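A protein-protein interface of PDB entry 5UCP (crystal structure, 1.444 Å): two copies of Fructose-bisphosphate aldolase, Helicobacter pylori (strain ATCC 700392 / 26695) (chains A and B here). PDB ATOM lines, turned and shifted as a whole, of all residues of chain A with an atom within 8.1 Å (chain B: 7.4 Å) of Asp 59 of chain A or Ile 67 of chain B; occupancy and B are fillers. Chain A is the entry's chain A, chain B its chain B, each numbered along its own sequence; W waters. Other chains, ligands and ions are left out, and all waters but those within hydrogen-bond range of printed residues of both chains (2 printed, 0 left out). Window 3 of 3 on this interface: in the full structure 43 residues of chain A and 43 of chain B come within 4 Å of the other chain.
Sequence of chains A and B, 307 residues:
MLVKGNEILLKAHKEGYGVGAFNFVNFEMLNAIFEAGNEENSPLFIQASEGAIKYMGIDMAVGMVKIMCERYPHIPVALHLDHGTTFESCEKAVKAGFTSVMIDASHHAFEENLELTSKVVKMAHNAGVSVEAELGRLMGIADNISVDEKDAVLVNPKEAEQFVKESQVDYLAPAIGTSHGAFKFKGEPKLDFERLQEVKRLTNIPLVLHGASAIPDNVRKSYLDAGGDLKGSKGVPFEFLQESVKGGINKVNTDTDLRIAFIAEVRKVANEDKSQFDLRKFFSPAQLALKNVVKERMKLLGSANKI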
ATOM      1  N   ILE A  53     -15.369  -7.099   5.359  1.00  0.00           N
ATOM      2  CA  ILE A  53     -14.448  -6.288   6.150  1.00  0.00           C
ATOM      3  C   ILE A  53     -14.392  -4.855   5.621  1.00  0.00           C
ATOM      4  O   ILE A  53     -14.398  -3.888   6.401  1.00  0.00           O
ATOM      5  CB  ILE A  53     -13.064  -6.954   6.221  1.00  0.00           C
ATOM      6  CG1 ILE A  53     -13.163  -8.225   7.075  1.00  0.00           C
ATOM      7  CG2 ILE A  53     -12.037  -5.990   6.800  1.00  0.00           C
ATOM      8  CD1 ILE A  53     -11.917  -9.117   7.043  1.00  0.00           C
ATOM      9  N   LYS A  54     -14.375  -4.685   4.297  1.00  0.00           N
ATOM     10  CA  LYS A  54     -14.391  -3.339   3.722  1.00  0.00           C
ATOM     11  C   LYS A  54     -15.676  -2.605   4.100  1.00  0.00           C
ATOM     12  O   LYS A  54     -15.652  -1.405   4.396  1.00  0.00           O
ATOM     13  CB  LYS A  54     -14.257  -3.416   2.201  1.00  0.00           C
ATOM     14  CG  LYS A  54     -13.987  -2.063   1.530  1.00  0.00           C
ATOM     15  CD  LYS A  54     -13.808  -2.194   0.021  1.00  0.00           C
ATOM     16  CE  LYS A  54     -12.568  -3.006  -0.348  1.00  0.00           C
ATOM     17  NZ  LYS A  54     -11.314  -2.431   0.219  1.00  0.00           N
ATOM     18  N   TYR A  55     -16.803  -3.313   4.082  1.00  0.00           N
ATOM     19  CA  TYR A  55     -18.104  -2.724   4.389  1.00  0.00           C
ATOM     20  C   TYR A  55     -18.198  -2.309   5.853  1.00  0.00           C
ATOM     21  O   TYR A  55     -18.630  -1.190   6.161  1.00  0.00           O
ATOM     22  CB  TYR A  55     -19.168  -3.754   4.026  1.00  0.00           C
ATOM     23  CG  TYR A  55     -20.579  -3.348   4.314  1.00  0.00           C
ATOM     24  CD1 TYR A  55     -21.283  -2.543   3.425  1.00  0.00           C
ATOM     25  CD2 TYR A  55     -21.219  -3.786   5.463  1.00  0.00           C
ATOM     26  CE1 TYR A  55     -22.592  -2.182   3.683  1.00  0.00           C
ATOM     27  CE2 TYR A  55     -22.520  -3.421   5.737  1.00  0.00           C
ATOM     28  CZ  TYR A  55     -23.201  -2.623   4.836  1.00  0.00           C
ATOM     29  OH  TYR A  55     -24.502  -2.260   5.086  1.00  0.00           O
ATOM     30  N   MET A  56     -17.813  -3.198   6.775  1.00  0.00           N
ATOM     31  CA  MET A  56     -17.944  -2.918   8.204  1.00  0.00           C
ATOM     32  C   MET A  56     -16.785  -2.096   8.739  1.00  0.00           C
ATOM     33  O   MET A  56     -16.971  -1.315   9.681  1.00  0.00           O
ATOM     34  CB  MET A  56     -18.000  -4.224   9.008  1.00  0.00           C
ATOM     35  CG  MET A  56     -19.277  -5.008   8.867  1.00  0.00           C
ATOM     36  SD  MET A  56     -19.258  -6.539   9.841  1.00  0.00           S
ATOM     37  CE  MET A  56     -18.278  -7.570   8.759  1.00  0.00           C
ATOM     38  N   GLY A  57     -15.599  -2.239   8.149  1.00  0.00           N
ATOM     39  CA  GLY A  57     -14.362  -1.845   8.792  1.00  0.00           C
ATOM     40  C   GLY A  57     -13.884  -2.976   9.679  1.00  0.00           C
ATOM     41  O   GLY A  57     -14.675  -3.544  10.434  1.00  0.00           O
ATOM     42  N   ILE A  58     -12.595  -3.323   9.602  1.00  0.00           N
ATOM     43  CA  ILE A  58     -12.097  -4.471  10.356  1.00  0.00           C
ATOM     44  C   ILE A  58     -12.240  -4.253  11.863  1.00  0.00           C
ATOM     45  O   ILE A  58     -12.456  -5.209  12.621  1.00  0.00           O
ATOM     46  CB  ILE A  58     -10.656  -4.800   9.915  1.00  0.00           C
ATOM     47  CG1 ILE A  58     -10.336  -6.244  10.290  1.00  0.00           C
ATOM     48  CG2 ILE A  58      -9.639  -3.863  10.544  1.00  0.00           C
ATOM     49  CD1 ILE A  58      -9.093  -6.798   9.592  1.00  0.00           C
ATOM     50  N   ASP A  59     -12.146  -2.997  12.321  1.00  0.00           N
ATOM     51  CA  ASP A  59     -12.308  -2.690  13.738  1.00  0.00           C
ATOM     52  C   ASP A  59     -13.721  -2.994  14.227  1.00  0.00           C
ATOM     53  O   ASP A  59     -13.908  -3.428  15.373  1.00  0.00           O
ATOM     54  CB  ASP A  59     -11.936  -1.218  13.981  1.00  0.00           C
ATOM     55  CG  ASP A  59     -12.708  -0.231  13.068  1.00  0.00           C
ATOM     56  OD1 ASP A  59     -12.995   0.913  13.504  1.00  0.00           O
ATOM     57  OD2 ASP A  59     -13.043  -0.575  11.913  1.00  0.00           O
ATOM     58  N   MET A  60     -14.721  -2.785  13.378  1.00  0.00           N
ATOM     59  CA  MET A  60     -16.098  -3.078  13.769  1.00  0.00           C
ATOM     60  C   MET A  60     -16.407  -4.562  13.647  1.00  0.00           C
ATOM     61  O   MET A  60     -17.154  -5.118  14.464  1.00  0.00           O
ATOM     62  CB  MET A  60     -17.060  -2.256  12.911  1.00  0.00           C
ATOM     63  CG  MET A  60     -18.520  -2.422  13.250  1.00  0.00           C
ATOM     64  SD  MET A  60     -18.965  -1.772  14.869  1.00  0.00           S
ATOM     65  CE  MET A  60     -18.851  -0.003  14.573  1.00  0.00           C
ATOM     66  N   ALA A  61     -15.852  -5.218  12.632  1.00  0.00           N
ATOM     67  CA  ALA A  61     -16.058  -6.651  12.493  1.00  0.00           C
ATOM     68  C   ALA A  61     -15.559  -7.385  13.728  1.00  0.00           C
ATOM     69  O   ALA A  61     -16.288  -8.187  14.321  1.00  0.00           O
ATOM     70  CB  ALA A  61     -15.362  -7.170  11.236  1.00  0.00           C
ATOM     71  N   VAL A  62     -14.318  -7.110  14.138  1.00  0.00           N
ATOM     72  CA  VAL A  62     -13.772  -7.738  15.333  1.00  0.00           C
ATOM     73  C   VAL A  62     -14.522  -7.269  16.572  1.00  0.00           C
ATOM     74  O   VAL A  62     -14.857  -8.067  17.451  1.00  0.00           O
ATOM     75  CB  VAL A  62     -12.263  -7.470  15.444  1.00  0.00           C
ATOM     76  CG1 VAL A  62     -11.742  -8.048  16.753  1.00  0.00           C
ATOM     77  CG2 VAL A  62     -11.511  -8.062  14.230  1.00  0.00           C
ATOM     78  N   GLY A  63     -14.787  -5.963  16.663  1.00  0.00           N
ATOM     79  CA  GLY A  63     -15.396  -5.409  17.865  1.00  0.00           C
ATOM     80  C   GLY A  63     -16.780  -5.973  18.138  1.00  0.00           C
ATOM     81  O   GLY A  63     -17.107  -6.322  19.275  1.00  0.00           O
ATOM     82  N   MET A  64     -17.619  -6.065  17.100  1.00  0.00           N
ATOM     83  CA  MET A  64     -18.944  -6.644  17.288  1.00  0.00           C
ATOM     84  C   MET A  64     -18.858  -8.098  17.735  1.00  0.00           C
ATOM     85  O   MET A  64     -19.613  -8.530  18.614  1.00  0.00           O
ATOM     86  CB  MET A  64     -19.782  -6.539  16.010  1.00  0.00           C
ATOM     87  CG  MET A  64     -20.266  -5.127  15.674  1.00  0.00           C
ATOM     88  SD  MET A  64     -21.582  -5.116  14.410  1.00  0.00           S
ATOM     89  CE  MET A  64     -20.788  -5.992  13.082  1.00  0.00           C
ATOM     90  N   VAL A  65     -17.952  -8.875  17.135  1.00  0.00           N
ATOM     91  CA  VAL A  65     -17.832 -10.276  17.526  1.00  0.00           C
ATOM     92  C   VAL A  65     -17.384 -10.395  18.977  1.00  0.00           C
ATOM     93  O   VAL A  65     -17.899 -11.230  19.733  1.00  0.00           O
ATOM     94  CB  VAL A  65     -16.908 -11.045  16.557  1.00  0.00           C
ATOM     95  CG1 VAL A  65     -16.644 -12.438  17.064  1.00  0.00           C
ATOM     96  CG2 VAL A  65     -17.531 -11.075  15.175  1.00  0.00           C
ATOM     97  N   LYS A  66     -16.428  -9.561  19.398  1.00  0.00           N
ATOM     98  CA  LYS A  66     -15.977  -9.610  20.785  1.00  0.00           C
ATOM     99  C   LYS A  66     -17.108  -9.277  21.762  1.00  0.00           C
ATOM    100  O   LYS A  66     -17.229  -9.908  22.814  1.00  0.00           O
ATOM    101  CB  LYS A  66     -14.767  -8.699  20.982  1.00  0.00           C
ATOM    102  CG  LYS A  66     -13.479  -9.287  20.395  1.00  0.00           C
ATOM    103  CD  LYS A  66     -12.253  -8.409  20.642  1.00  0.00           C
ATOM    104  CE  LYS A  66     -10.973  -9.090  20.148  1.00  0.00           C
ATOM    105  NZ  LYS A  66      -9.754  -8.250  20.346  1.00  0.00           N
ATOM    106  N   ILE A  67     -17.960  -8.306  21.423  1.00  0.00           N
ATOM    107  CA  ILE A  67     -19.130  -8.010  22.247  1.00  0.00           C
ATOM    108  C   ILE A  67     -20.054  -9.223  22.326  1.00  0.00           C
ATOM    109  O   ILE A  67     -20.564  -9.565  23.406  1.00  0.00           O
ATOM    110  CB  ILE A  67     -19.862  -6.779  21.688  1.00  0.00           C
ATOM    111  CG1 ILE A  67     -19.001  -5.536  21.891  1.00  0.00           C
ATOM    112  CG2 ILE A  67     -21.220  -6.600  22.353  1.00  0.00           C
ATOM    113  CD1 ILE A  67     -19.401  -4.385  21.020  1.00  0.00           C
ATOM    114  N   ALA A  96      -5.678  -7.399  13.769  1.00  0.00           N
ATOM    115  CA  ALA A  96      -6.949  -6.885  14.270  1.00  0.00           C
ATOM    116  C   ALA A  96      -7.615  -7.797  15.299  1.00  0.00           C
ATOM    117  O   ALA A  96      -8.504  -7.334  16.022  1.00  0.00           O
ATOM    118  CB  ALA A  96      -7.912  -6.649  13.105  1.00  0.00           C
ATOM    119  N   PHE A  98      -8.474 -11.435  14.517  1.00  0.00           N
ATOM    120  CA  PHE A  98      -9.026 -12.676  13.994  1.00  0.00           C
ATOM    121  C   PHE A  98      -8.248 -13.857  14.571  1.00  0.00           C
ATOM    122  O   PHE A  98      -7.054 -13.759  14.866  1.00  0.00           O
ATOM    123  CB  PHE A  98      -8.930 -12.702  12.469  1.00  0.00           C
ATOM    124  CG  PHE A  98     -10.004 -11.925  11.774  1.00  0.00           C
ATOM    125  CD1 PHE A  98     -10.056 -10.538  11.867  1.00  0.00           C
ATOM    126  CD2 PHE A  98     -10.964 -12.574  11.023  1.00  0.00           C
ATOM    127  CE1 PHE A  98     -11.053  -9.824  11.220  1.00  0.00           C
ATOM    128  CE2 PHE A  98     -11.969 -11.875  10.382  1.00  0.00           C
ATOM    129  CZ  PHE A  98     -12.011 -10.494  10.472  1.00  0.00           C
ATOM    130  N   PHE B  27     -25.865  -0.990  12.845  1.00  0.00           N
ATOM    131  CA  PHE B  27     -24.573  -0.515  12.355  1.00  0.00           C
ATOM    132  C   PHE B  27     -24.732   0.424  11.166  1.00  0.00           C
ATOM    133  O   PHE B  27     -24.063   1.456  11.093  1.00  0.00           O
ATOM    134  CB  PHE B  27     -23.655  -1.686  11.980  1.00  0.00           C
ATOM    135  CG  PHE B  27     -22.496  -1.278  11.101  1.00  0.00           C
ATOM    136  CD1 PHE B  27     -21.445  -0.553  11.637  1.00  0.00           C
ATOM    137  CD2 PHE B  27     -22.492  -1.550   9.746  1.00  0.00           C
ATOM    138  CE1 PHE B  27     -20.391  -0.141  10.852  1.00  0.00           C
ATOM    139  CE2 PHE B  27     -21.439  -1.138   8.952  1.00  0.00           C
ATOM    140  CZ  PHE B  27     -20.389  -0.418   9.514  1.00  0.00           C
ATOM    141  N   LEU B  30     -25.686   3.901  12.216  1.00  0.00           N
ATOM    142  CA  LEU B  30     -24.616   4.529  12.975  1.00  0.00           C
ATOM    143  C   LEU B  30     -23.465   4.940  12.074  1.00  0.00           C
ATOM    144  O   LEU B  30     -22.918   6.039  12.212  1.00  0.00           O
ATOM    145  CB  LEU B  30     -24.148   3.588  14.072  1.00  0.00           C
ATOM    146  CG  LEU B  30     -23.158   4.132  15.084  1.00  0.00           C
ATOM    147  CD1 LEU B  30     -23.807   5.212  15.908  1.00  0.00           C
ATOM    148  CD2 LEU B  30     -22.670   3.021  15.978  1.00  0.00           C
ATOM    149  N   PHE B  34     -22.039   8.854  11.467  1.00  0.00           N
ATOM    150  CA  PHE B  34     -20.658   9.246  11.747  1.00  0.00           C
ATOM    151  C   PHE B  34     -19.963   9.796  10.506  1.00  0.00           C
ATOM    152  O   PHE B  34     -19.238  10.790  10.587  1.00  0.00           O
ATOM    153  CB  PHE B  34     -19.874   8.065  12.311  1.00  0.00           C
ATOM    154  CG  PHE B  34     -19.823   8.043  13.803  1.00  0.00           C
ATOM    155  CD1 PHE B  34     -20.882   7.538  14.541  1.00  0.00           C
ATOM    156  CD2 PHE B  34     -18.721   8.544  14.477  1.00  0.00           C
ATOM    157  CE1 PHE B  34     -20.841   7.520  15.925  1.00  0.00           C
ATOM    158  CE2 PHE B  34     -18.673   8.524  15.857  1.00  0.00           C
ATOM    159  CZ  PHE B  34     -19.740   8.020  16.584  1.00  0.00           C
ATOM    160  N   MET B  60     -24.176  -3.813  23.018  1.00  0.00           N
ATOM    161  CA  MET B  60     -23.827  -3.592  21.619  1.00  0.00           C
ATOM    162  C   MET B  60     -24.039  -2.139  21.216  1.00  0.00           C
ATOM    163  O   MET B  60     -23.255  -1.580  20.438  1.00  0.00           O
ATOM    164  CB  MET B  60     -24.655  -4.511  20.724  1.00  0.00           C
ATOM    165  CG  MET B  60     -24.293  -4.402  19.239  1.00  0.00           C
ATOM    166  SD  MET B  60     -22.620  -4.935  18.810  1.00  0.00           S
ATOM    167  CE  MET B  60     -22.768  -6.702  19.045  1.00  0.00           C
ATOM    168  N   ALA B  61     -25.085  -1.502  21.743  1.00  0.00           N
ATOM    169  CA  ALA B  61     -25.294  -0.090  21.463  1.00  0.00           C
ATOM    170  C   ALA B  61     -24.084   0.725  21.887  1.00  0.00           C
ATOM    171  O   ALA B  61     -23.509   1.476  21.090  1.00  0.00           O
ATOM    172  CB  ALA B  61     -26.548   0.398  22.190  1.00  0.00           C
ATOM    173  N   VAL B  62     -23.669   0.577  23.143  1.00  0.00           N
ATOM    174  CA  VAL B  62     -22.510   1.322  23.612  1.00  0.00           C
ATOM    175  C   VAL B  62     -21.256   0.878  22.877  1.00  0.00           C
ATOM    176  O   VAL B  62     -20.432   1.704  22.469  1.00  0.00           O
ATOM    177  CB  VAL B  62     -22.375   1.168  25.136  1.00  0.00           C
ATOM    178  CG1 VAL B  62     -21.101   1.852  25.611  1.00  0.00           C
ATOM    179  CG2 VAL B  62     -23.614   1.739  25.864  1.00  0.00           C
ATOM    180  N   GLY B  63     -21.085  -0.438  22.702  1.00  0.00           N
ATOM    181  CA  GLY B  63     -19.868  -0.952  22.093  1.00  0.00           C
ATOM    182  C   GLY B  63     -19.637  -0.457  20.679  1.00  0.00           C
ATOM    183  O   GLY B  63     -18.519  -0.072  20.323  1.00  0.00           O
ATOM    184  N   MET B  64     -20.689  -0.447  19.849  1.00  0.00           N
ATOM    185  CA  MET B  64     -20.530   0.047  18.488  1.00  0.00           C
ATOM    186  C   MET B  64     -20.178   1.527  18.483  1.00  0.00           C
ATOM    187  O   MET B  64     -19.335   1.970  17.699  1.00  0.00           O
ATOM    188  CB  MET B  64     -21.792  -0.201  17.657  1.00  0.00           C
ATOM    189  CG  MET B  64     -22.042  -1.652  17.296  1.00  0.00           C
ATOM    190  SD  MET B  64     -23.297  -1.867  16.011  1.00  0.00           S
ATOM    191  CE  MET B  64     -24.669  -0.966  16.685  1.00  0.00           C
ATOM    192  N   VAL B  65     -20.792   2.314  19.364  1.00  0.00           N
ATOM    193  CA  VAL B  65     -20.485   3.733  19.379  1.00  0.00           C
ATOM    194  C   VAL B  65     -19.044   3.981  19.810  1.00  0.00           C
ATOM    195  O   VAL B  65     -18.368   4.862  19.261  1.00  0.00           O
ATOM    196  CB  VAL B  65     -21.503   4.481  20.254  1.00  0.00           C
ATOM    197  CG1 VAL B  65     -21.112   5.945  20.409  1.00  0.00           C
ATOM    198  CG2 VAL B  65     -22.883   4.360  19.639  1.00  0.00           C
ATOM    199  N   LYS B  66     -18.551   3.226  20.790  1.00  0.00           N
ATOM    200  CA  LYS B  66     -17.161   3.389  21.210  1.00  0.00           C
ATOM    201  C   LYS B  66     -16.185   3.032  20.089  1.00  0.00           C
ATOM    202  O   LYS B  66     -15.164   3.703  19.916  1.00  0.00           O
ATOM    203  CB  LYS B  66     -16.899   2.579  22.474  1.00  0.00           C
ATOM    204  CG  LYS B  66     -17.454   3.235  23.723  1.00  0.00           C
ATOM    205  CD  LYS B  66     -17.222   2.388  24.971  1.00  0.00           C
ATOM    206  CE  LYS B  66     -17.677   3.131  26.232  1.00  0.00           C
ATOM    207  NZ  LYS B  66     -17.505   2.323  27.479  1.00  0.00           N
ATOM    208  N   ILE B  67     -16.497   2.004  19.296  1.00  0.00           N
ATOM    209  CA  ILE B  67     -15.664   1.674  18.135  1.00  0.00           C
ATOM    210  C   ILE B  67     -15.660   2.832  17.135  1.00  0.00           C
ATOM    211  O   ILE B  67     -14.611   3.212  16.587  1.00  0.00           O
ATOM    212  CB  ILE B  67     -16.149   0.364  17.489  1.00  0.00           C
ATOM    213  CG1 ILE B  67     -15.915  -0.817  18.435  1.00  0.00           C
ATOM    214  CG2 ILE B  67     -15.455   0.130  16.139  1.00  0.00           C
ATOM    215  CD1 ILE B  67     -16.805  -1.982  18.151  1.00  0.00           C
ATOM    216  N   MET B  68     -16.839   3.401  16.876  1.00  0.00           N
ATOM    217  CA  MET B  68     -16.946   4.501  15.927  1.00  0.00           C
ATOM    218  C   MET B  68     -16.215   5.748  16.421  1.00  0.00           C
ATOM    219  O   MET B  68     -15.577   6.450  15.629  1.00  0.00           O
ATOM    220  CB  MET B  68     -18.415   4.788  15.625  1.00  0.00           C
ATOM    221  CG  MET B  68     -19.128   3.648  14.891  1.00  0.00           C
ATOM    222  SD  MET B  68     -18.387   3.221  13.291  1.00  0.00           S
ATOM    223  CE  MET B  68     -18.583   4.749  12.383  1.00  0.00           C
ATOM    224  N   CYS B  69     -16.271   6.038  17.719  1.00  0.00           N
ATOM    225  CA  CYS B  69     -15.565   7.221  18.197  1.00  0.00           C
ATOM    226  C   CYS B  69     -14.053   7.038  18.139  1.00  0.00           C
ATOM    227  O   CYS B  69     -13.319   8.016  17.954  1.00  0.00           O
ATOM    228  CB  CYS B  69     -16.039   7.604  19.601  1.00  0.00           C
ATOM    229  SG  CYS B  69     -15.221   6.742  20.940  1.00  0.00           S
ATOM    230  N   GLU B  70     -13.562   5.805  18.285  1.00  0.00           N
ATOM    231  CA  GLU B  70     -12.130   5.562  18.100  1.00  0.00           C
ATOM    232  C   GLU B  70     -11.729   5.651  16.630  1.00  0.00           C
ATOM    233  O   GLU B  70     -10.586   6.002  16.310  1.00  0.00           O
ATOM    234  CB  GLU B  70     -11.748   4.200  18.681  1.00  0.00           C
ATOM    235  CG  GLU B  70     -11.891   4.091  20.192  1.00  0.00           C
ATOM    236  CD  GLU B  70     -11.599   2.692  20.705  1.00  0.00           C
ATOM    237  OE1 GLU B  70     -11.634   1.740  19.897  1.00  0.00           O
ATOM    238  OE2 GLU B  70     -11.334   2.545  21.916  1.00  0.00           O
ATOM    239  N   ARG B  71     -12.651   5.336  15.724  1.00  0.00           N
ATOM    240  CA  ARG B  71     -12.389   5.494  14.300  1.00  0.00           C
ATOM    241  C   ARG B  71     -12.317   6.967  13.913  1.00  0.00           C
ATOM    242  O   ARG B  71     -11.568   7.330  12.999  1.00  0.00           O
ATOM    243  CB  ARG B  71     -13.484   4.750  13.524  1.00  0.00           C
ATOM    244  CG  ARG B  71     -13.357   4.747  12.045  1.00  0.00           C
ATOM    245  CD  ARG B  71     -14.576   4.106  11.397  1.00  0.00           C
ATOM    246  NE  ARG B  71     -14.673   2.664  11.628  1.00  0.00           N
ATOM    247  CZ  ARG B  71     -15.559   1.876  11.024  1.00  0.00           C
ATOM    248  NH1 ARG B  71     -16.420   2.377  10.150  1.00  0.00           N
ATOM    249  NH2 ARG B  71     -15.585   0.573  11.282  1.00  0.00           N
ATOM    250  N   TYR B  72     -13.067   7.831  14.607  1.00  0.00           N
ATOM    251  CA  TYR B  72     -13.112   9.271  14.322  1.00  0.00           C
ATOM    252  C   TYR B  72     -12.857  10.053  15.605  1.00  0.00           C
ATOM    253  O   TYR B  72     -13.762  10.709  16.141  1.00  0.00           O
ATOM    254  CB  TYR B  72     -14.465   9.676  13.741  1.00  0.00           C
ATOM    255  CG  TYR B  72     -14.828   9.030  12.435  1.00  0.00           C
ATOM    256  CD1 TYR B  72     -15.725   7.978  12.386  1.00  0.00           C
ATOM    257  CD2 TYR B  72     -14.300   9.500  11.248  1.00  0.00           C
ATOM    258  CE1 TYR B  72     -16.079   7.390  11.178  1.00  0.00           C
ATOM    259  CE2 TYR B  72     -14.635   8.920  10.034  1.00  0.00           C
ATOM    260  CZ  TYR B  72     -15.524   7.862  10.004  1.00  0.00           C
ATOM    261  OH  TYR B  72     -15.866   7.291   8.796  1.00  0.00           O
HETATM  262  O   HOH W   1     -12.372   1.828  15.847  1.00  0.00           O
HETATM  263  O   HOH W   2     -17.293   1.012   7.500  1.00  0.00           O
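Water W1 lies within hydrogen-bond range of OD1 of Asp 59 of chain A and O of Ile 67 of chain B.
Water W2 lies within hydrogen-bond range of the backbone carbonyl oxygen of Tyr 55 of chain A (2.9 Å), the guanidinium group of Arg 71 of chain B (3.1 Å) and the backbone carbonyl oxygen of Met 56 of chain A (3.2 Å).
Printed residues of chain B within 4 Å of Gly 57 of chain A: Arg 71.
Of chain B, only Ile 67 and Arg 71 come within 4 Å of Asp 59 of chain A.
Of the printed residues of chain B, Met 60 of chain A touches Phe 27, Met 64, Ile 67, Met 68 and Arg 71.
Ala 61 of chain A touches none of the printed residues of chain B.
Of the printed residues of chain A, Gly 63 of chain B touches Ile 67.
Ile 67 of chain B touches just these residues of chain A: Asp 59 (3.7 Å), Met 60 (3.7 Å) and Gly 63 (3.7 Å).
The nearest residue of chain B that does not touch Asp 59 of chain A is Met 68 of chain B (5.7 Å).
The nearest residue of chain A that does not touch Ile 67 of chain B is Met 64 of chain A (4.3 Å).
The nearest printed residue of chain B that does not touch Met 56 of chain A is Met 68 of chain B (6.0 Å).
Met 60 of chain A touches Met 64 of chain B, and with the chains exchanged Met 64 of chain A touches Met 60 of chain B.
Met 60 of chain A touches Ile 67 of chain B, and with the chains exchanged Ile 67 of chain A touches Met 60 of chain B.
Gly 63 of chain A touches Ile 67 of chain B, and with the chains exchanged Ile 67 of chain A touches Gly 63 of chain B.
8 positions are printed for both chains.
The guanidinium group of Arg 71 of chain B lies within salt-bridge range of the side-chain carboxylate of Asp 59 of chain A (2.9 Å).
The guanidinium group (NH2) of Arg 71 of chain B lies within hydrogen-bond range of the backbone carbonyl oxygen (O) of Met 56 of chain A, 2.8 Å away.
Printed residues of chain B that touch a printed residue of chain A: Phe 27, Met 60, Gly 63, Met 64, Ile 67, Met 68 and Arg 71.
Of the 17 printed residues of chain A, 8 touch a printed residue of chain B.
Printed residues of chain A that touch a printed residue of chain B: Tyr 55, Met 56, Gly 57, Asp 59, Met 60, Gly 63, Met 64 and Ile 67.
Among the printed residues, Asp or Glu carboxylates within 4 Å of a Lys or Arg side-chain nitrogen of the other chain: Asp 59 of chain A with Arg 71 of chain B (2.9 Å).
Phe 27 of chain B touches Tyr 55 of chain A (CZ to O, 3.9 Å).
Phe 27 of chain B touches Met 56 of chain A (CZ to O, 3.5 Å).
Gly 57 of chain A touches Arg 71 of chain B (CA to NH2, 3.7 Å).
Asp 59 of chain A touches Ile 67 of chain B (OD1 to CG2, 3.7 Å).
Met 60 of chain A touches Met 64 of chain B.
Met 60 of chain A touches Met 68 of chain B.
CB of Met 60 of chain A touches NH2 of Arg 71 of chain B (3.6 Å).
Ile 67 of chain B touches Gly 63 of chain A.
Met 64 of chain A touches Met 60 of chain B.
Ile 67 of chain A touches Gly 63 of chain B (CD1 to CA, 3.6 Å).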
